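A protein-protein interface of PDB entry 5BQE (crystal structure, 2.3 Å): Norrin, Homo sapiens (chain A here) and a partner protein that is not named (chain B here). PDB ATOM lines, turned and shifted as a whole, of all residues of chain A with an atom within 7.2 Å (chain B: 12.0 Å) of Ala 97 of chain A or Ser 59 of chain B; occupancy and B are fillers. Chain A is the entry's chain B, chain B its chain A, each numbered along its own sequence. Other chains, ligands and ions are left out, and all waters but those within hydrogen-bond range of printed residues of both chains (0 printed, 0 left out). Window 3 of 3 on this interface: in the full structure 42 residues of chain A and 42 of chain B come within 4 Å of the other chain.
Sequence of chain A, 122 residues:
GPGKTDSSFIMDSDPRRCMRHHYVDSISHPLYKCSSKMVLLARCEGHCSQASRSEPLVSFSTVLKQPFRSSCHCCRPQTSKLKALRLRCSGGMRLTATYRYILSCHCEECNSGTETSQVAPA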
ATOM      1  N   ILE A  27     -10.267   0.478  19.282  1.00  0.00           N
ATOM      2  CA  ILE A  27      -9.121   1.072  19.927  1.00  0.00           C
ATOM      3  C   ILE A  27      -9.278   2.557  20.121  1.00  0.00           C
ATOM      4  O   ILE A  27      -9.638   3.255  19.214  1.00  0.00           O
ATOM      5  CB  ILE A  27      -7.870   0.846  19.094  1.00  0.00           C
ATOM      6  CG1 ILE A  27      -7.638  -0.630  18.881  1.00  0.00           C
ATOM      7  CG2 ILE A  27      -6.675   1.435  19.771  1.00  0.00           C
ATOM      8  CD1 ILE A  27      -7.831  -1.470  20.108  1.00  0.00           C
ATOM      9  N   HIS A  29      -7.273   6.060  21.938  1.00  0.00           N
ATOM     10  CA  HIS A  29      -6.133   6.661  22.625  1.00  0.00           C
ATOM     11  C   HIS A  29      -6.626   7.364  23.896  1.00  0.00           C
ATOM     12  O   HIS A  29      -7.552   8.174  23.825  1.00  0.00           O
ATOM     13  CB  HIS A  29      -5.409   7.643  21.700  1.00  0.00           C
ATOM     14  CG  HIS A  29      -4.002   7.954  22.110  1.00  0.00           C
ATOM     15  ND1 HIS A  29      -2.953   7.962  21.222  1.00  0.00           N
ATOM     16  CD2 HIS A  29      -3.479   8.283  23.318  1.00  0.00           C
ATOM     17  CE1 HIS A  29      -1.837   8.270  21.860  1.00  0.00           C
ATOM     18  NE2 HIS A  29      -2.128   8.468  23.132  1.00  0.00           N
ATOM     19  N   MLY A  83       2.669  -4.588  13.374  1.00  0.00           N
ATOM     20  CA  MLY A  83       1.643  -3.979  12.549  1.00  0.00           C
ATOM     21  CB  MLY A  83       0.421  -4.890  12.476  1.00  0.00           C
ATOM     22  CG  MLY A  83      -0.480  -4.607  11.296  1.00  0.00           C
ATOM     23  CD  MLY A  83      -1.387  -5.787  11.004  1.00  0.00           C
ATOM     24  CE  MLY A  83      -2.267  -5.516   9.801  1.00  0.00           C
ATOM     25  NZ  MLY A  83      -3.430  -6.441   9.743  1.00  0.00           N
ATOM     26  CH1 MLY A  83      -4.303  -5.923   8.683  1.00  0.00           C
ATOM     27  CH2 MLY A  83      -2.950  -7.759   9.300  1.00  0.00           C
ATOM     28  C   MLY A  83       1.289  -2.635  13.168  1.00  0.00           C
ATOM     29  O   MLY A  83       1.250  -2.501  14.391  1.00  0.00           O
ATOM     30  N   ALA A  84       1.040  -1.645  12.317  1.00  0.00           N
ATOM     31  CA  ALA A  84       0.852  -0.268  12.758  1.00  0.00           C
ATOM     32  C   ALA A  84      -0.600   0.166  12.600  1.00  0.00           C
ATOM     33  O   ALA A  84      -1.306  -0.305  11.708  1.00  0.00           O
ATOM     34  CB  ALA A  84       1.775   0.659  11.980  1.00  0.00           C
ATOM     35  N   LEU A  85      -1.036   1.068  13.474  1.00  0.00           N
ATOM     36  CA  LEU A  85      -2.406   1.563  13.455  1.00  0.00           C
ATOM     37  C   LEU A  85      -2.443   3.082  13.511  1.00  0.00           C
ATOM     38  O   LEU A  85      -2.322   3.674  14.583  1.00  0.00           O
ATOM     39  CB  LEU A  85      -3.196   0.983  14.626  1.00  0.00           C
ATOM     40  CG  LEU A  85      -4.685   1.322  14.667  1.00  0.00           C
ATOM     41  CD1 LEU A  85      -5.371   0.806  13.411  1.00  0.00           C
ATOM     42  CD2 LEU A  85      -5.336   0.740  15.916  1.00  0.00           C
ATOM     43  N   ARG A  86      -2.628   3.707  12.353  1.00  0.00           N
ATOM     44  CA  ARG A  86      -2.697   5.160  12.272  1.00  0.00           C
ATOM     45  C   ARG A  86      -4.069   5.610  12.762  1.00  0.00           C
ATOM     46  O   ARG A  86      -5.092   5.187  12.218  1.00  0.00           O
ATOM     47  CB  ARG A  86      -2.481   5.674  10.843  1.00  0.00           C
ATOM     48  CG  ARG A  86      -1.602   4.841   9.909  1.00  0.00           C
ATOM     49  CD  ARG A  86      -2.065   5.066   8.474  1.00  0.00           C
ATOM     50  NE  ARG A  86      -0.977   5.127   7.503  1.00  0.00           N
ATOM     51  CZ  ARG A  86      -1.128   5.539   6.247  1.00  0.00           C
ATOM     52  NH1 ARG A  86      -0.089   5.566   5.428  1.00  0.00           N
ATOM     53  NH2 ARG A  86      -2.319   5.930   5.810  1.00  0.00           N
ATOM     54  N   LEU A  87      -4.098   6.458  13.785  1.00  0.00           N
ATOM     55  CA  LEU A  87      -5.353   7.021  14.264  1.00  0.00           C
ATOM     56  C   LEU A  87      -5.684   8.321  13.542  1.00  0.00           C
ATOM     57  O   LEU A  87      -4.801   8.992  13.003  1.00  0.00           O
ATOM     58  CB  LEU A  87      -5.303   7.276  15.772  1.00  0.00           C
ATOM     59  CG  LEU A  87      -5.555   6.103  16.723  1.00  0.00           C
ATOM     60  CD1 LEU A  87      -5.517   6.604  18.158  1.00  0.00           C
ATOM     61  CD2 LEU A  87      -6.882   5.416  16.441  1.00  0.00           C
ATOM     62  N   LEU A  95      -1.816   9.889  15.360  1.00  0.00           N
ATOM     63  CA  LEU A  95      -1.093   9.062  16.313  1.00  0.00           C
ATOM     64  C   LEU A  95      -1.040   7.641  15.779  1.00  0.00           C
ATOM     65  O   LEU A  95      -1.899   7.237  14.996  1.00  0.00           O
ATOM     66  CB  LEU A  95      -1.762   9.119  17.687  1.00  0.00           C
ATOM     67  CG  LEU A  95      -1.884  10.554  18.208  1.00  0.00           C
ATOM     68  CD1 LEU A  95      -2.883  10.646  19.343  1.00  0.00           C
ATOM     69  CD2 LEU A  95      -0.521  11.083  18.635  1.00  0.00           C
ATOM     70  N   THR A  96      -0.028   6.889  16.197  1.00  0.00           N
ATOM     71  CA  THR A  96       0.208   5.562  15.643  1.00  0.00           C
ATOM     72  C   THR A  96       0.373   4.531  16.749  1.00  0.00           C
ATOM     73  O   THR A  96       1.314   4.602  17.541  1.00  0.00           O
ATOM     74  CB  THR A  96       1.462   5.544  14.740  1.00  0.00           C
ATOM     75  OG1 THR A  96       1.285   6.462  13.654  1.00  0.00           O
ATOM     76  CG2 THR A  96       1.717   4.146  14.177  1.00  0.00           C
ATOM     77  N   ALA A  97      -0.552   3.576  16.797  1.00  0.00           N
ATOM     78  CA  ALA A  97      -0.435   2.446  17.708  1.00  0.00           C
ATOM     79  C   ALA A  97       0.259   1.295  16.998  1.00  0.00           C
ATOM     80  O   ALA A  97       0.236   1.209  15.769  1.00  0.00           O
ATOM     81  CB  ALA A  97      -1.798   2.006  18.216  1.00  0.00           C
ATOM     82  N   THR A  98       0.841   0.397  17.760  1.00  0.00           N
ATOM     83  CA  THR A  98       1.396  -0.815  17.195  1.00  0.00           C
ATOM     84  C   THR A  98       1.035  -2.015  18.034  1.00  0.00           C
ATOM     85  O   THR A  98       0.642  -1.881  19.176  1.00  0.00           O
ATOM     86  CB  THR A  98       2.914  -0.763  17.137  1.00  0.00           C
ATOM     87  OG1 THR A  98       3.407  -0.256  18.371  1.00  0.00           O
ATOM     88  CG2 THR A  98       3.343   0.127  16.052  1.00  0.00           C
ATOM     89  N   TYR A  99       1.193  -3.190  17.450  1.00  0.00           N
ATOM     90  CA  TYR A  99       0.900  -4.417  18.130  1.00  0.00           C
ATOM     91  C   TYR A  99       1.333  -5.550  17.261  1.00  0.00           C
ATOM     92  O   TYR A  99       1.612  -5.356  16.117  1.00  0.00           O
ATOM     93  CB  TYR A  99      -0.579  -4.509  18.358  1.00  0.00           C
ATOM     94  CG  TYR A  99      -1.349  -4.537  17.094  1.00  0.00           C
ATOM     95  CD1 TYR A  99      -1.759  -3.382  16.496  1.00  0.00           C
ATOM     96  CD2 TYR A  99      -1.676  -5.719  16.494  1.00  0.00           C
ATOM     97  CE1 TYR A  99      -2.475  -3.406  15.335  1.00  0.00           C
ATOM     98  CE2 TYR A  99      -2.392  -5.751  15.330  1.00  0.00           C
ATOM     99  CZ  TYR A  99      -2.790  -4.583  14.764  1.00  0.00           C
ATOM    100  OH  TYR A  99      -3.497  -4.596  13.613  1.00  0.00           O
ATOM    101  N   GLU B  55      -3.210 -13.032  23.560  1.00  0.00           N
ATOM    102  CA  GLU B  55      -3.768 -11.913  22.809  1.00  0.00           C
ATOM    103  C   GLU B  55      -2.724 -10.820  22.628  1.00  0.00           C
ATOM    104  O   GLU B  55      -1.902 -10.603  23.516  1.00  0.00           O
ATOM    105  CB  GLU B  55      -4.989 -11.342  23.534  1.00  0.00           C
ATOM    106  CG  GLU B  55      -6.259 -12.167  23.392  1.00  0.00           C
ATOM    107  CD  GLU B  55      -7.303 -11.820  24.438  1.00  0.00           C
ATOM    108  OE1 GLU B  55      -7.144 -10.790  25.124  1.00  0.00           O
ATOM    109  OE2 GLU B  55      -8.282 -12.584  24.573  1.00  0.00           O
ATOM    110  N   PRO B  56      -2.766 -10.095  21.540  1.00  0.00           N
ATOM    111  CA  PRO B  56      -1.863  -8.969  21.409  1.00  0.00           C
ATOM    112  C   PRO B  56      -2.324  -7.821  22.262  1.00  0.00           C
ATOM    113  O   PRO B  56      -3.494  -7.658  22.466  1.00  0.00           O
ATOM    114  CB  PRO B  56      -1.998  -8.601  19.957  1.00  0.00           C
ATOM    115  CG  PRO B  56      -3.356  -9.020  19.613  1.00  0.00           C
ATOM    116  CD  PRO B  56      -3.515 -10.316  20.310  1.00  0.00           C
ATOM    117  N   LEU B  57      -1.385  -7.040  22.756  1.00  0.00           N
ATOM    118  CA  LEU B  57      -1.686  -5.812  23.454  1.00  0.00           C
ATOM    119  C   LEU B  57      -1.370  -4.691  22.523  1.00  0.00           C
ATOM    120  O   LEU B  57      -0.430  -4.767  21.780  1.00  0.00           O
ATOM    121  CB  LEU B  57      -0.837  -5.696  24.698  1.00  0.00           C
ATOM    122  CG  LEU B  57      -1.176  -6.686  25.792  1.00  0.00           C
ATOM    123  CD1 LEU B  57      -0.100  -6.720  26.845  1.00  0.00           C
ATOM    124  CD2 LEU B  57      -2.493  -6.329  26.423  1.00  0.00           C
ATOM    125  N   VAL B  58      -2.164  -3.645  22.553  1.00  0.00           N
ATOM    126  CA  VAL B  58      -1.950  -2.535  21.648  1.00  0.00           C
ATOM    127  C   VAL B  58      -1.281  -1.382  22.361  1.00  0.00           C
ATOM    128  O   VAL B  58      -1.708  -0.992  23.420  1.00  0.00           O
ATOM    129  CB  VAL B  58      -3.253  -2.069  21.028  1.00  0.00           C
ATOM    130  CG1 VAL B  58      -3.030  -0.855  20.170  1.00  0.00           C
ATOM    131  CG2 VAL B  58      -3.832  -3.171  20.201  1.00  0.00           C
ATOM    132  N   SER B  59      -0.225  -0.850  21.769  1.00  0.00           N
ATOM    133  CA  SER B  59       0.533   0.214  22.402  1.00  0.00           C
ATOM    134  C   SER B  59       0.688   1.460  21.565  1.00  0.00           C
ATOM    135  O   SER B  59       1.081   1.416  20.422  1.00  0.00           O
ATOM    136  CB  SER B  59       1.912  -0.293  22.777  1.00  0.00           C
ATOM    137  OG  SER B  59       2.677   0.738  23.338  1.00  0.00           O
ATOM    138  N   PHE B  60       0.386   2.591  22.165  1.00  0.00           N
ATOM    139  CA  PHE B  60       0.704   3.853  21.545  1.00  0.00           C
ATOM    140  C   PHE B  60       2.056   4.363  21.976  1.00  0.00           C
ATOM    141  O   PHE B  60       2.657   5.190  21.329  1.00  0.00           O
ATOM    142  CB  PHE B  60      -0.334   4.853  21.935  1.00  0.00           C
ATOM    143  CG  PHE B  60      -1.639   4.607  21.317  1.00  0.00           C
ATOM    144  CD1 PHE B  60      -1.841   4.921  20.007  1.00  0.00           C
ATOM    145  CD2 PHE B  60      -2.651   4.055  22.036  1.00  0.00           C
ATOM    146  CE1 PHE B  60      -3.051   4.706  19.418  1.00  0.00           C
ATOM    147  CE2 PHE B  60      -3.867   3.835  21.462  1.00  0.00           C
ATOM    148  CZ  PHE B  60      -4.067   4.163  20.149  1.00  0.00           C
ATOM    149  N   SER B  61       2.571   3.792  23.036  1.00  0.00           N
ATOM    150  CA  SER B  61       3.689   4.375  23.707  1.00  0.00           C
ATOM    151  C   SER B  61       4.879   4.004  22.892  1.00  0.00           C
ATOM    152  O   SER B  61       4.761   3.676  21.730  1.00  0.00           O
ATOM    153  CB  SER B  61       3.791   3.857  25.140  1.00  0.00           C
ATOM    154  OG  SER B  61       4.696   2.783  25.286  1.00  0.00           O
ATOM    155  N   THR B  62       6.040   4.144  23.483  1.00  0.00           N
ATOM    156  CA  THR B  62       7.251   3.808  22.795  1.00  0.00           C
ATOM    157  C   THR B  62       7.172   2.356  22.461  1.00  0.00           C
ATOM    158  O   THR B  62       6.812   1.567  23.327  1.00  0.00           O
ATOM    159  CB  THR B  62       8.410   3.934  23.772  1.00  0.00           C
ATOM    160  OG1 THR B  62       8.177   3.051  24.872  1.00  0.00           O
ATOM    161  CG2 THR B  62       8.483   5.358  24.290  1.00  0.00           C
ATOM    162  N   VAL B  63       7.505   2.005  21.221  1.00  0.00           N
ATOM    163  CA  VAL B  63       7.742   0.622  20.844  1.00  0.00           C
ATOM    164  C   VAL B  63       6.563  -0.208  21.315  1.00  0.00           C
ATOM    165  O   VAL B  63       5.444   0.170  21.093  1.00  0.00           O
ATOM    166  CB  VAL B  63       9.080   0.082  21.386  1.00  0.00           C
ATOM    167  CG1 VAL B  63       9.048   0.005  22.906  1.00  0.00           C
ATOM    168  CG2 VAL B  63       9.333  -1.302  20.814  1.00  0.00           C
ATOM    169  N   LEU B  64       6.822  -1.300  22.014  1.00  0.00           N
ATOM    170  CA  LEU B  64       5.807  -2.101  22.655  1.00  0.00           C
ATOM    171  C   LEU B  64       6.519  -2.610  23.889  1.00  0.00           C
ATOM    172  O   LEU B  64       7.721  -2.545  23.938  1.00  0.00           O
ATOM    173  CB  LEU B  64       5.383  -3.259  21.745  1.00  0.00           C
ATOM    174  CG  LEU B  64       4.076  -3.175  20.948  1.00  0.00           C
ATOM    175  CD1 LEU B  64       4.108  -4.102  19.753  1.00  0.00           C
ATOM    176  CD2 LEU B  64       2.875  -3.493  21.809  1.00  0.00           C
ATOM    177  N   LYS B  65       5.826  -3.152  24.876  1.00  0.00           N
ATOM    178  CA  LYS B  65       6.541  -3.619  26.056  1.00  0.00           C
ATOM    179  C   LYS B  65       6.588  -5.129  26.127  1.00  0.00           C
ATOM    180  O   LYS B  65       7.546  -5.755  25.696  1.00  0.00           O
ATOM    181  CB  LYS B  65       5.869  -3.092  27.315  1.00  0.00           C
ATOM    182  CG  LYS B  65       6.384  -1.743  27.763  1.00  0.00           C
ATOM    183  CD  LYS B  65       7.878  -1.784  27.972  1.00  0.00           C
ATOM    184  CE  LYS B  65       8.304  -0.833  29.078  1.00  0.00           C
ATOM    185  NZ  LYS B  65       8.733  -1.541  30.316  1.00  0.00           N
ATOM    186  N   GLN B  66       5.535  -5.702  26.676  1.00  0.00           N
ATOM    187  CA  GLN B  66       5.295  -7.105  26.582  1.00  0.00           C
ATOM    188  C   GLN B  66       4.221  -7.183  25.538  1.00  0.00           C
ATOM    189  O   GLN B  66       3.155  -6.634  25.701  1.00  0.00           O
ATOM    190  CB  GLN B  66       4.802  -7.616  27.916  1.00  0.00           C
ATOM    191  CG  GLN B  66       4.049  -8.918  27.850  1.00  0.00           C
ATOM    192  CD  GLN B  66       4.845 -10.015  27.188  1.00  0.00           C
ATOM    193  OE1 GLN B  66       4.295 -10.843  26.452  1.00  0.00           O
ATOM    194  NE2 GLN B  66       6.150 -10.038  27.454  1.00  0.00           N
ATOM    195  N   PRO B  67       4.582  -7.893  24.390  1.00  0.00           N
ATOM    196  CA  PRO B  67       3.597  -7.812  23.315  1.00  0.00           C
ATOM    197  C   PRO B  67       2.278  -8.532  23.542  1.00  0.00           C
ATOM    198  O   PRO B  67       1.315  -8.169  22.929  1.00  0.00           O
ATOM    199  CB  PRO B  67       4.331  -8.365  22.119  1.00  0.00           C
ATOM    200  CG  PRO B  67       5.164  -9.404  22.667  1.00  0.00           C
ATOM    201  CD  PRO B  67       5.741  -8.761  23.850  1.00  0.00           C
ATOM    202  N   PHE B  68       2.243  -9.548  24.380  1.00  0.00           N
ATOM    203  CA  PHE B  68       1.056 -10.355  24.500  1.00  0.00           C
ATOM    204  C   PHE B  68       0.566 -10.459  25.909  1.00  0.00           C
ATOM    205  O   PHE B  68       1.305 -10.304  26.823  1.00  0.00           O
ATOM    206  CB  PHE B  68       1.322 -11.748  23.979  1.00  0.00           C
ATOM    207  CG  PHE B  68       1.840 -11.783  22.589  1.00  0.00           C
ATOM    208  CD1 PHE B  68       0.998 -11.629  21.532  1.00  0.00           C
ATOM    209  CD2 PHE B  68       3.159 -11.982  22.349  1.00  0.00           C
ATOM    210  CE1 PHE B  68       1.465 -11.666  20.263  1.00  0.00           C
ATOM    211  CE2 PHE B  68       3.643 -12.020  21.082  1.00  0.00           C
ATOM    212  CZ  PHE B  68       2.792 -11.864  20.032  1.00  0.00           C
ATOM    213  N   ARG B  69      -0.706 -10.747  26.046  1.00  0.00           N
ATOM    214  CA  ARG B  69      -1.322 -10.994  27.313  1.00  0.00           C
ATOM    215  C   ARG B  69      -1.921 -12.373  27.242  1.00  0.00           C
ATOM    216  O   ARG B  69      -2.679 -12.649  26.366  1.00  0.00           O
ATOM    217  CB  ARG B  69      -2.418  -9.984  27.541  1.00  0.00           C
ATOM    218  CG  ARG B  69      -3.257 -10.258  28.760  1.00  0.00           C
ATOM    219  CD  ARG B  69      -4.696  -9.846  28.561  1.00  0.00           C
ATOM    220  NE  ARG B  69      -4.830  -8.437  28.225  1.00  0.00           N
ATOM    221  CZ  ARG B  69      -5.792  -7.950  27.452  1.00  0.00           C
ATOM    222  NH1 ARG B  69      -6.704  -8.764  26.943  1.00  0.00           N
ATOM    223  NH2 ARG B  69      -5.845  -6.655  27.190  1.00  0.00           N
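The backbone carbonyl oxygen of Ser 59 of chain B is in hydrogen-bond range of the backbone NH of Thr 98 of chain A, at 2.9 Å.
O of Val 63 of chain B lies within hydrogen-bond range of OG1 of Thr 98 of chain A, 3.4 Å away.
The backbone carbonyl oxygen of Pro 67 of chain B sits at hydrogen-bond distance from the backbone NH of Leu 57 of chain B, at 2.9 Å.
OG of Ser 59 of chain B sits at hydrogen-bond distance from N of Ser 61 of chain B (3.1 Å).
N of MLY 83 of chain A sits at hydrogen-bond distance from O of Tyr 99 of chain A, 3.0 Å away.
N of Leu 85 of chain A is in hydrogen-bond range of O of Ala 97 of chain A.
N of Leu 87 of chain A lies within hydrogen-bond range of O of Leu 95 of chain A, at 2.6 Å.
Among the printed residues, merely in contact across the chains: Ala 97 of chain A with Phe 60 of chain B (3.2 Å), Ala 97 of chain A with Ser 59 of chain B (3.3 Å), Leu 87 of chain A with Phe 60 of chain B (3.4 Å), Tyr 99 of chain A with Leu 57 of chain B (3.4 Å), His 29 of chain A with Phe 60 of chain B (3.5 Å), Tyr 99 of chain A with Leu 64 of chain B (3.6 Å), Thr 98 of chain A with Val 58 of chain B (3.6 Å), Ala 97 of chain A with Val 58 of chain B (3.7 Å), Ile 27 of chain A with Phe 60 of chain B (3.8 Å), Thr 98 of chain A with Leu 64 of chain B (3.8 Å), Thr 96 of chain A with Phe 60 of chain B (3.96 Å) and Tyr 99 of chain A with Val 58 of chain B (3.97 Å).
Printed residues of chain B within 4 Å of Ile 27 of chain A: Phe 60 (3.8 Å).
Printed residues of chain B within 4 Å of His 29 of chain A: Phe 60.
No residue of chain B comes within 4 Å of Ala 84 of chain A.
Leu 85 of chain A touches none of the printed residues of chain B.
Of chain B, only Phe 60 (3.4 Å) comes within 4 Å of Leu 87 of chain A.
No residue of chain B comes within 4 Å of Leu 95 of chain A.
Of chain B, only Val 58, Ser 59, Val 63 and Leu 64 come within 4 Å of Thr 98 of chain A.
Of chain B, only Leu 57 (3.4 Å), Val 58 (3.97 Å) and Leu 64 (3.6 Å) come within 4 Å of Tyr 99 of chain A.
Printed residues of chain A within 4 Å of Leu 57 of chain B: Tyr 99 (3.4 Å).
Printed residues of chain A within 4 Å of Val 58 of chain B: Ala 97, Thr 98 and Tyr 99.
Printed residues of chain A within 4 Å of Ser 59 of chain B: Ala 97 and Thr 98.
Of the printed residues of chain A, Leu 64 of chain B touches Thr 98 (3.8 Å) and Tyr 99 (3.6 Å).
The nearest residue of chain B that does not touch Ala 97 of chain A is Ser 61 of chain B (6.3 Å).
Printed residues of chain B that touch a printed residue of chain A: Leu 57, Val 58, Ser 59, Phe 60, Val 63 and Leu 64.
Hydrophobic or aromatic side chains of chain B that line the printed part of chain A: Val 58, Phe 60 and Leu 64.
Printed residues of chain A that touch a printed residue of chain B: Ile 27, His 29, Leu 87, Thr 96, Ala 97, Thr 98 and Tyr 99.
Hydrophobic or aromatic side chains of chain A that line the printed part of chain B: Ile 27, His 29, Leu 87, Ala 97 and Tyr 99.
Among the printed residues, 14 pairs touch across the chains.
Among the printed residues, no Asp or Glu carboxylate lies within 4 Å of a Lys or Arg side-chain nitrogen of the other chain.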
